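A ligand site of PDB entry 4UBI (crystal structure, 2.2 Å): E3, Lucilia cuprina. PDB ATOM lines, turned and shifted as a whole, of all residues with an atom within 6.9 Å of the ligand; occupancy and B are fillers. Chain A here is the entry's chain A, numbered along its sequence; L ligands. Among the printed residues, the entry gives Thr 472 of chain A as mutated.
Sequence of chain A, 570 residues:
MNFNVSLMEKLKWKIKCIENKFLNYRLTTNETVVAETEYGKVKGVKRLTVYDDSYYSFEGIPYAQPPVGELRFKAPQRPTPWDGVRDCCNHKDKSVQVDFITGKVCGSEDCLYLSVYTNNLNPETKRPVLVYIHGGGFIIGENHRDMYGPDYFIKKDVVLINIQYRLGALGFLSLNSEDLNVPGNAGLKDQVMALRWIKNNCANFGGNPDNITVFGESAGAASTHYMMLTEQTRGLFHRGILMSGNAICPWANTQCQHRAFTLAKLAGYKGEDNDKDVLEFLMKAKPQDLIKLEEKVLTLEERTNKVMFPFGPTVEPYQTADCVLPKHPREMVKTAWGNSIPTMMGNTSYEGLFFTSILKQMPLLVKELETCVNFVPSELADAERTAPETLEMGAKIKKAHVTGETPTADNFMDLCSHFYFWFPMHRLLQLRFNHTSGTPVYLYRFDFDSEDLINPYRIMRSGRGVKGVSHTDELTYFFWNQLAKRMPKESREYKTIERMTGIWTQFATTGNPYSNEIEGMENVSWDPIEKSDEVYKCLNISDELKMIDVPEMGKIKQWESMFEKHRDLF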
ATOM      1  N   HIS A 134       5.803  -8.738   0.183  1.00  0.00           N
ATOM      2  CA  HIS A 134       4.647  -8.190   0.882  1.00  0.00           C
ATOM      3  C   HIS A 134       3.352  -8.796   0.350  1.00  0.00           C
ATOM      4  O   HIS A 134       3.304  -9.334  -0.762  1.00  0.00           O
ATOM      5  CB  HIS A 134       4.624  -6.678   0.770  1.00  0.00           C
ATOM      6  CG  HIS A 134       4.303  -6.185  -0.622  1.00  0.00           C
ATOM      7  ND1 HIS A 134       3.016  -6.117  -1.100  1.00  0.00           N
ATOM      8  CD2 HIS A 134       5.103  -5.723  -1.604  1.00  0.00           C
ATOM      9  CE1 HIS A 134       3.034  -5.636  -2.335  1.00  0.00           C
ATOM     10  NE2 HIS A 134       4.292  -5.402  -2.668  1.00  0.00           N
ATOM     11  N   GLY A 135       2.301  -8.729   1.182  1.00  0.00           N
ATOM     12  CA  GLY A 135       0.963  -9.134   0.813  1.00  0.00           C
ATOM     13  C   GLY A 135       0.143  -7.902   0.453  1.00  0.00           C
ATOM     14  O   GLY A 135       0.698  -6.802   0.299  1.00  0.00           O
ATOM     15  N   GLY A 136      -1.167  -8.080   0.350  1.00  0.00           N
ATOM     16  CA  GLY A 136      -2.050  -7.052  -0.165  1.00  0.00           C
ATOM     17  C   GLY A 136      -2.893  -7.574  -1.316  1.00  0.00           C
ATOM     18  O   GLY A 136      -3.201  -6.857  -2.262  1.00  0.00           O
ATOM     19  N   GLY A 137      -3.270  -8.849  -1.231  1.00  0.00           N
ATOM     20  CA  GLY A 137      -4.158  -9.469  -2.197  1.00  0.00           C
ATOM     21  C   GLY A 137      -3.741  -9.341  -3.651  1.00  0.00           C
ATOM     22  O   GLY A 137      -4.593  -9.507  -4.537  1.00  0.00           O
ATOM     23  N   PHE A 138      -2.453  -9.092  -3.892  1.00  0.00           N
ATOM     24  CA  PHE A 138      -1.910  -8.775  -5.224  1.00  0.00           C
ATOM     25  C   PHE A 138      -2.439  -7.440  -5.810  1.00  0.00           C
ATOM     26  O   PHE A 138      -2.223  -7.137  -6.976  1.00  0.00           O
ATOM     27  CB  PHE A 138      -2.185  -9.920  -6.224  1.00  0.00           C
ATOM     28  CG  PHE A 138      -1.646 -11.266  -5.783  1.00  0.00           C
ATOM     29  CD1 PHE A 138      -0.305 -11.581  -5.955  1.00  0.00           C
ATOM     30  CD2 PHE A 138      -2.489 -12.206  -5.188  1.00  0.00           C
ATOM     31  CE1 PHE A 138       0.192 -12.819  -5.527  1.00  0.00           C
ATOM     32  CE2 PHE A 138      -1.999 -13.456  -4.760  1.00  0.00           C
ATOM     33  CZ  PHE A 138      -0.659 -13.763  -4.938  1.00  0.00           C
ATOM     34  N   ILE A 140      -2.605  -4.358  -3.503  1.00  0.00           N
ATOM     35  CA  ILE A 140      -1.951  -3.271  -2.747  1.00  0.00           C
ATOM     36  C   ILE A 140      -0.665  -3.790  -2.114  1.00  0.00           C
ATOM     37  O   ILE A 140      -0.410  -4.998  -2.117  1.00  0.00           O
ATOM     38  CB  ILE A 140      -2.835  -2.674  -1.628  1.00  0.00           C
ATOM     39  CG1 ILE A 140      -3.140  -3.737  -0.562  1.00  0.00           C
ATOM     40  CG2 ILE A 140      -4.093  -2.004  -2.199  1.00  0.00           C
ATOM     41  CD1 ILE A 140      -3.726  -3.179   0.715  1.00  0.00           C
ATOM     42  N   GLU A 217       3.695 -12.776   3.790  1.00  0.00           N
ATOM     43  CA  GLU A 217       2.437 -12.944   4.512  1.00  0.00           C
ATOM     44  C   GLU A 217       1.237 -12.684   3.587  1.00  0.00           C
ATOM     45  O   GLU A 217       1.253 -11.742   2.793  1.00  0.00           O
ATOM     46  CB  GLU A 217       2.427 -12.024   5.735  1.00  0.00           C
ATOM     47  CG  GLU A 217       1.182 -12.105   6.604  1.00  0.00           C
ATOM     48  CD  GLU A 217       0.154 -11.055   6.250  1.00  0.00           C
ATOM     49  OE1 GLU A 217       0.518 -10.073   5.562  1.00  0.00           O
ATOM     50  OE2 GLU A 217      -1.014 -11.215   6.663  1.00  0.00           O
ATOM     51  N   SER A 218       0.218 -13.538   3.681  1.00  0.00           N
ATOM     52  CA  SER A 218      -1.012 -13.415   2.879  1.00  0.00           C
ATOM     53  C   SER A 218      -0.704 -13.596   1.390  1.00  0.00           C
ATOM     54  O   SER A 218      -0.181 -14.631   0.998  1.00  0.00           O
ATOM     55  CB  SER A 218      -1.706 -12.089   3.152  1.00  0.00           C
ATOM     56  OG  SER A 218      -3.072 -12.157   2.823  1.00  0.00           O
ATOM     57  N   ALA A 219      -1.005 -12.599   0.556  1.00  0.00           N
ATOM     58  CA  ALA A 219      -0.638 -12.667  -0.862  1.00  0.00           C
ATOM     59  C   ALA A 219       0.879 -12.848  -1.018  1.00  0.00           C
ATOM     60  O   ALA A 219       1.339 -13.411  -2.014  1.00  0.00           O
ATOM     61  CB  ALA A 219      -1.109 -11.422  -1.609  1.00  0.00           C
ATOM     62  N   GLY A 220       1.660 -12.412  -0.025  1.00  0.00           N
ATOM     63  CA  GLY A 220       3.095 -12.594  -0.063  1.00  0.00           C
ATOM     64  C   GLY A 220       3.473 -14.017   0.283  1.00  0.00           C
ATOM     65  O   GLY A 220       4.486 -14.544  -0.168  1.00  0.00           O
ATOM     66  N   ALA A 221       2.653 -14.655   1.111  1.00  0.00           N
ATOM     67  CA  ALA A 221       2.829 -16.064   1.377  1.00  0.00           C
ATOM     68  C   ALA A 221       2.506 -16.897   0.126  1.00  0.00           C
ATOM     69  O   ALA A 221       3.261 -17.795  -0.252  1.00  0.00           O
ATOM     70  CB  ALA A 221       1.977 -16.486   2.570  1.00  0.00           C
ATOM     71  N   SER A 244       0.396 -17.275   6.873  1.00  0.00           N
ATOM     72  CA  SER A 244      -1.034 -17.099   6.593  1.00  0.00           C
ATOM     73  C   SER A 244      -1.319 -17.104   5.100  1.00  0.00           C
ATOM     74  O   SER A 244      -1.940 -16.167   4.597  1.00  0.00           O
ATOM     75  CB  SER A 244      -1.576 -15.797   7.191  1.00  0.00           C
ATOM     76  OG  SER A 244      -1.383 -15.730   8.591  1.00  0.00           O
ATOM     77  N   TRP A 251      -8.387 -17.690  -2.717  1.00  0.00           N
ATOM     78  CA  TRP A 251      -8.112 -16.328  -3.167  1.00  0.00           C
ATOM     79  C   TRP A 251      -6.777 -16.159  -3.931  1.00  0.00           C
ATOM     80  O   TRP A 251      -6.529 -15.098  -4.504  1.00  0.00           O
ATOM     81  CB  TRP A 251      -8.132 -15.364  -1.965  1.00  0.00           C
ATOM     82  CG  TRP A 251      -7.246 -15.825  -0.833  1.00  0.00           C
ATOM     83  CD1 TRP A 251      -7.619 -16.594   0.249  1.00  0.00           C
ATOM     84  CD2 TRP A 251      -5.832 -15.597  -0.686  1.00  0.00           C
ATOM     85  NE1 TRP A 251      -6.537 -16.841   1.063  1.00  0.00           N
ATOM     86  CE2 TRP A 251      -5.422 -16.234   0.514  1.00  0.00           C
ATOM     87  CE3 TRP A 251      -4.877 -14.915  -1.447  1.00  0.00           C
ATOM     88  CZ2 TRP A 251      -4.106 -16.213   0.959  1.00  0.00           C
ATOM     89  CZ3 TRP A 251      -3.569 -14.883  -1.002  1.00  0.00           C
ATOM     90  CH2 TRP A 251      -3.194 -15.534   0.199  1.00  0.00           C
ATOM     91  N   MET A 308     -12.436 -13.400  -4.716  1.00  0.00           N
ATOM     92  CA  MET A 308     -12.072 -12.217  -3.959  1.00  0.00           C
ATOM     93  C   MET A 308     -11.511 -11.095  -4.840  1.00  0.00           C
ATOM     94  O   MET A 308     -11.778  -9.916  -4.590  1.00  0.00           O
ATOM     95  CB  MET A 308     -11.060 -12.583  -2.880  1.00  0.00           C
ATOM     96  CG  MET A 308     -10.677 -11.411  -2.015  1.00  0.00           C
ATOM     97  SD  MET A 308      -9.846 -11.977  -0.526  1.00  0.00           S
ATOM     98  CE  MET A 308     -11.194 -12.764   0.343  1.00  0.00           C
ATOM     99  N   PHE A 309     -10.752 -11.449  -5.868  1.00  0.00           N
ATOM    100  CA  PHE A 309     -10.112 -10.445  -6.720  1.00  0.00           C
ATOM    101  C   PHE A 309     -10.327 -10.753  -8.208  1.00  0.00           C
ATOM    102  O   PHE A 309     -10.327 -11.923  -8.611  1.00  0.00           O
ATOM    103  CB  PHE A 309      -8.620 -10.359  -6.435  1.00  0.00           C
ATOM    104  CG  PHE A 309      -8.286 -10.157  -4.978  1.00  0.00           C
ATOM    105  CD1 PHE A 309      -8.489  -8.928  -4.370  1.00  0.00           C
ATOM    106  CD2 PHE A 309      -7.709 -11.187  -4.245  1.00  0.00           C
ATOM    107  CE1 PHE A 309      -8.165  -8.728  -3.022  1.00  0.00           C
ATOM    108  CE2 PHE A 309      -7.377 -10.998  -2.898  1.00  0.00           C
ATOM    109  CZ  PHE A 309      -7.602  -9.751  -2.277  1.00  0.00           C
ATOM    110  N   PHE A 354     -10.169 -10.506  10.754  1.00  0.00           N
ATOM    111  CA  PHE A 354      -9.930  -9.530   9.712  1.00  0.00           C
ATOM    112  C   PHE A 354     -11.200  -9.064   8.979  1.00  0.00           C
ATOM    113  O   PHE A 354     -11.245  -7.961   8.434  1.00  0.00           O
ATOM    114  CB  PHE A 354      -8.936 -10.111   8.711  1.00  0.00           C
ATOM    115  CG  PHE A 354      -8.505  -9.143   7.667  1.00  0.00           C
ATOM    116  CD1 PHE A 354      -9.161  -9.078   6.453  1.00  0.00           C
ATOM    117  CD2 PHE A 354      -7.432  -8.296   7.901  1.00  0.00           C
ATOM    118  CE1 PHE A 354      -8.773  -8.168   5.491  1.00  0.00           C
ATOM    119  CE2 PHE A 354      -7.029  -7.394   6.943  1.00  0.00           C
ATOM    120  CZ  PHE A 354      -7.700  -7.330   5.730  1.00  0.00           C
ATOM    121  N   PHE A 355     -12.232  -9.894   8.964  1.00  0.00           N
ATOM    122  CA  PHE A 355     -13.429  -9.606   8.172  1.00  0.00           C
ATOM    123  C   PHE A 355     -14.517  -8.872   8.943  1.00  0.00           C
ATOM    124  O   PHE A 355     -15.626  -8.719   8.445  1.00  0.00           O
ATOM    125  CB  PHE A 355     -13.986 -10.909   7.586  1.00  0.00           C
ATOM    126  CG  PHE A 355     -13.059 -11.553   6.608  1.00  0.00           C
ATOM    127  CD1 PHE A 355     -13.073 -11.173   5.278  1.00  0.00           C
ATOM    128  CD2 PHE A 355     -12.122 -12.480   7.032  1.00  0.00           C
ATOM    129  CE1 PHE A 355     -12.184 -11.744   4.379  1.00  0.00           C
ATOM    130  CE2 PHE A 355     -11.226 -13.046   6.138  1.00  0.00           C
ATOM    131  CZ  PHE A 355     -11.259 -12.689   4.814  1.00  0.00           C
ATOM    132  N   TYR A 420     -10.334 -19.524   4.208  1.00  0.00           N
ATOM    133  CA  TYR A 420      -9.282 -18.750   3.573  1.00  0.00           C
ATOM    134  C   TYR A 420      -7.888 -19.202   3.967  1.00  0.00           C
ATOM    135  O   TYR A 420      -6.934 -18.923   3.252  1.00  0.00           O
ATOM    136  CB  TYR A 420      -9.467 -17.266   3.910  1.00  0.00           C
ATOM    137  CG  TYR A 420     -10.694 -16.673   3.255  1.00  0.00           C
ATOM    138  CD1 TYR A 420     -10.745 -16.511   1.874  1.00  0.00           C
ATOM    139  CD2 TYR A 420     -11.795 -16.295   3.999  1.00  0.00           C
ATOM    140  CE1 TYR A 420     -11.875 -15.982   1.237  1.00  0.00           C
ATOM    141  CE2 TYR A 420     -12.933 -15.755   3.380  1.00  0.00           C
ATOM    142  CZ  TYR A 420     -12.962 -15.604   1.998  1.00  0.00           C
ATOM    143  OH  TYR A 420     -14.072 -15.054   1.373  1.00  0.00           O
ATOM    144  N   PHE A 421      -7.746 -19.902   5.087  1.00  0.00           N
ATOM    145  CA  PHE A 421      -6.392 -20.129   5.553  1.00  0.00           C
ATOM    146  C   PHE A 421      -6.081 -21.545   6.045  1.00  0.00           C
ATOM    147  O   PHE A 421      -5.198 -22.188   5.491  1.00  0.00           O
ATOM    148  CB  PHE A 421      -6.064 -19.107   6.652  1.00  0.00           C
ATOM    149  CG  PHE A 421      -6.079 -17.664   6.163  1.00  0.00           C
ATOM    150  CD1 PHE A 421      -5.085 -17.191   5.319  1.00  0.00           C
ATOM    151  CD2 PHE A 421      -7.087 -16.799   6.560  1.00  0.00           C
ATOM    152  CE1 PHE A 421      -5.111 -15.885   4.877  1.00  0.00           C
ATOM    153  CE2 PHE A 421      -7.106 -15.498   6.130  1.00  0.00           C
ATOM    154  CZ  PHE A 421      -6.118 -15.037   5.286  1.00  0.00           C
ATOM    155  N   TYR A 457      -2.658  -2.111   8.802  1.00  0.00           N
ATOM    156  CA  TYR A 457      -3.776  -2.981   8.413  1.00  0.00           C
ATOM    157  C   TYR A 457      -4.916  -2.966   9.432  1.00  0.00           C
ATOM    158  O   TYR A 457      -6.063  -3.253   9.089  1.00  0.00           O
ATOM    159  CB  TYR A 457      -3.305  -4.426   8.224  1.00  0.00           C
ATOM    160  CG  TYR A 457      -2.687  -4.731   6.890  1.00  0.00           C
ATOM    161  CD1 TYR A 457      -3.466  -4.827   5.739  1.00  0.00           C
ATOM    162  CD2 TYR A 457      -1.314  -4.968   6.777  1.00  0.00           C
ATOM    163  CE1 TYR A 457      -2.887  -5.129   4.504  1.00  0.00           C
ATOM    164  CE2 TYR A 457      -0.735  -5.270   5.560  1.00  0.00           C
ATOM    165  CZ  TYR A 457      -1.528  -5.351   4.432  1.00  0.00           C
ATOM    166  OH  TYR A 457      -0.949  -5.654   3.215  1.00  0.00           O
ATOM    167  N   MET A 460      -7.626  -0.655   8.415  1.00  0.00           N
ATOM    168  CA  MET A 460      -8.432  -1.093   7.278  1.00  0.00           C
ATOM    169  C   MET A 460      -9.451  -2.148   7.684  1.00  0.00           C
ATOM    170  O   MET A 460     -10.600  -2.110   7.253  1.00  0.00           O
ATOM    171  CB  MET A 460      -7.516  -1.619   6.171  1.00  0.00           C
ATOM    172  CG  MET A 460      -8.250  -2.305   5.030  1.00  0.00           C
ATOM    173  SD  MET A 460      -7.166  -3.462   4.148  1.00  0.00           S
ATOM    174  CE  MET A 460      -5.706  -2.454   3.941  1.00  0.00           C
ATOM    175  N   HIS A 471      -5.564 -11.894  11.253  1.00  0.00           N
ATOM    176  CA  HIS A 471      -4.741 -11.884  10.077  1.00  0.00           C
ATOM    177  C   HIS A 471      -4.038 -10.503  10.003  1.00  0.00           C
ATOM    178  O   HIS A 471      -4.710  -9.485  10.134  1.00  0.00           O
ATOM    179  CB  HIS A 471      -5.632 -12.144   8.855  1.00  0.00           C
ATOM    180  CG  HIS A 471      -4.879 -12.217   7.564  1.00  0.00           C
ATOM    181  ND1 HIS A 471      -3.992 -13.228   7.288  1.00  0.00           N
ATOM    182  CD2 HIS A 471      -4.892 -11.407   6.484  1.00  0.00           C
ATOM    183  CE1 HIS A 471      -3.473 -13.035   6.081  1.00  0.00           C
ATOM    184  NE2 HIS A 471      -4.005 -11.936   5.575  1.00  0.00           N
ATOM    185  N   THR A 472      -2.709 -10.512   9.857  1.00  0.00           N
ATOM    186  CA  THR A 472      -1.780  -9.338   9.804  1.00  0.00           C
ATOM    187  C   THR A 472      -1.360  -8.743  11.154  1.00  0.00           C
ATOM    188  O   THR A 472      -0.570  -7.794  11.180  1.00  0.00           O
ATOM    189  CB  THR A 472      -2.314  -8.140   8.977  1.00  0.00           C
ATOM    190  OG1 THR A 472      -3.309  -7.428   9.722  1.00  0.00           O
ATOM    191  CG2 THR A 472      -2.858  -8.562   7.612  1.00  0.00           C
ATOM    192  N   LEU A 475       2.621  -8.877  11.737  1.00  0.00           N
ATOM    193  CA  LEU A 475       3.573  -8.037  11.015  1.00  0.00           C
ATOM    194  C   LEU A 475       4.213  -6.993  11.909  1.00  0.00           C
ATOM    195  O   LEU A 475       5.385  -6.656  11.761  1.00  0.00           O
ATOM    196  CB  LEU A 475       2.885  -7.349   9.837  1.00  0.00           C
ATOM    197  CG  LEU A 475       2.450  -8.271   8.703  1.00  0.00           C
ATOM    198  CD1 LEU A 475       1.606  -7.515   7.682  1.00  0.00           C
ATOM    199  CD2 LEU A 475       3.663  -8.911   8.057  1.00  0.00           C
HETATM  200  O1  LIG L   1      -2.722 -10.515   0.975  1.00  0.00           O
HETATM  201  P1  LIG L   1      -3.706 -11.082   1.949  1.00  0.00           P
HETATM  202  O2  LIG L   1      -4.933 -11.701   1.062  1.00  0.00           O
HETATM  203  C1  LIG L   1      -5.554 -12.821   1.576  1.00  0.00           C
HETATM  204  C2  LIG L   1      -7.038 -12.659   1.372  1.00  0.00           C
HETATM  205  O3  LIG L   1      -4.433  -9.800   2.702  1.00  0.00           O
HETATM  206  C3  LIG L   1      -3.686  -9.085   3.612  1.00  0.00           C
HETATM  207  C4  LIG L   1      -4.598  -8.139   4.356  1.00  0.00           C
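O1 of the ligand is in hydrogen-bond range of N of Ala 219 (2.7 Å). The backbone NH (N) of Gly 136 is in hydrogen-bond range of an oxygen (O1) of the ligand. P1 of the ligand is covalently linked to OG of Ser 218 (1.5 Å). N of Gly 137 is in hydrogen-bond range of O1 of the ligand, at 2.8 Å.
NE2 of His 471 lies close to OE2 of Glu 217. NE1 of Trp 251 sits at hydrogen-bond distance from O of Tyr 420 (3.0 Å). A ring nitrogen (NE2) of His 471 lies within hydrogen-bond range of the side-chain hydroxyl (OG) of Ser 218 (2.9 Å).
Residues that only touch the ligand: Met 308 (3.5 Å), Tyr 457 (3.5 Å), His 471 (3.5 Å), Phe 354 (3.5 Å), Trp 251 (3.6 Å), Thr 472 (3.7 Å) and Gly 135 (3.9 Å). Hydrophobic or aromatic side chains within 4 Å of the ligand: Ala 219, Trp 251, Met 308, Phe 354, Tyr 457 and His 471. 11 residues have an atom within 4 Å of the ligand: Gly 135, Gly 136, Gly 137, Ser 218, Ala 219, Trp 251, Met 308, Phe 354, Tyr 457, His 471 and Thr 472.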
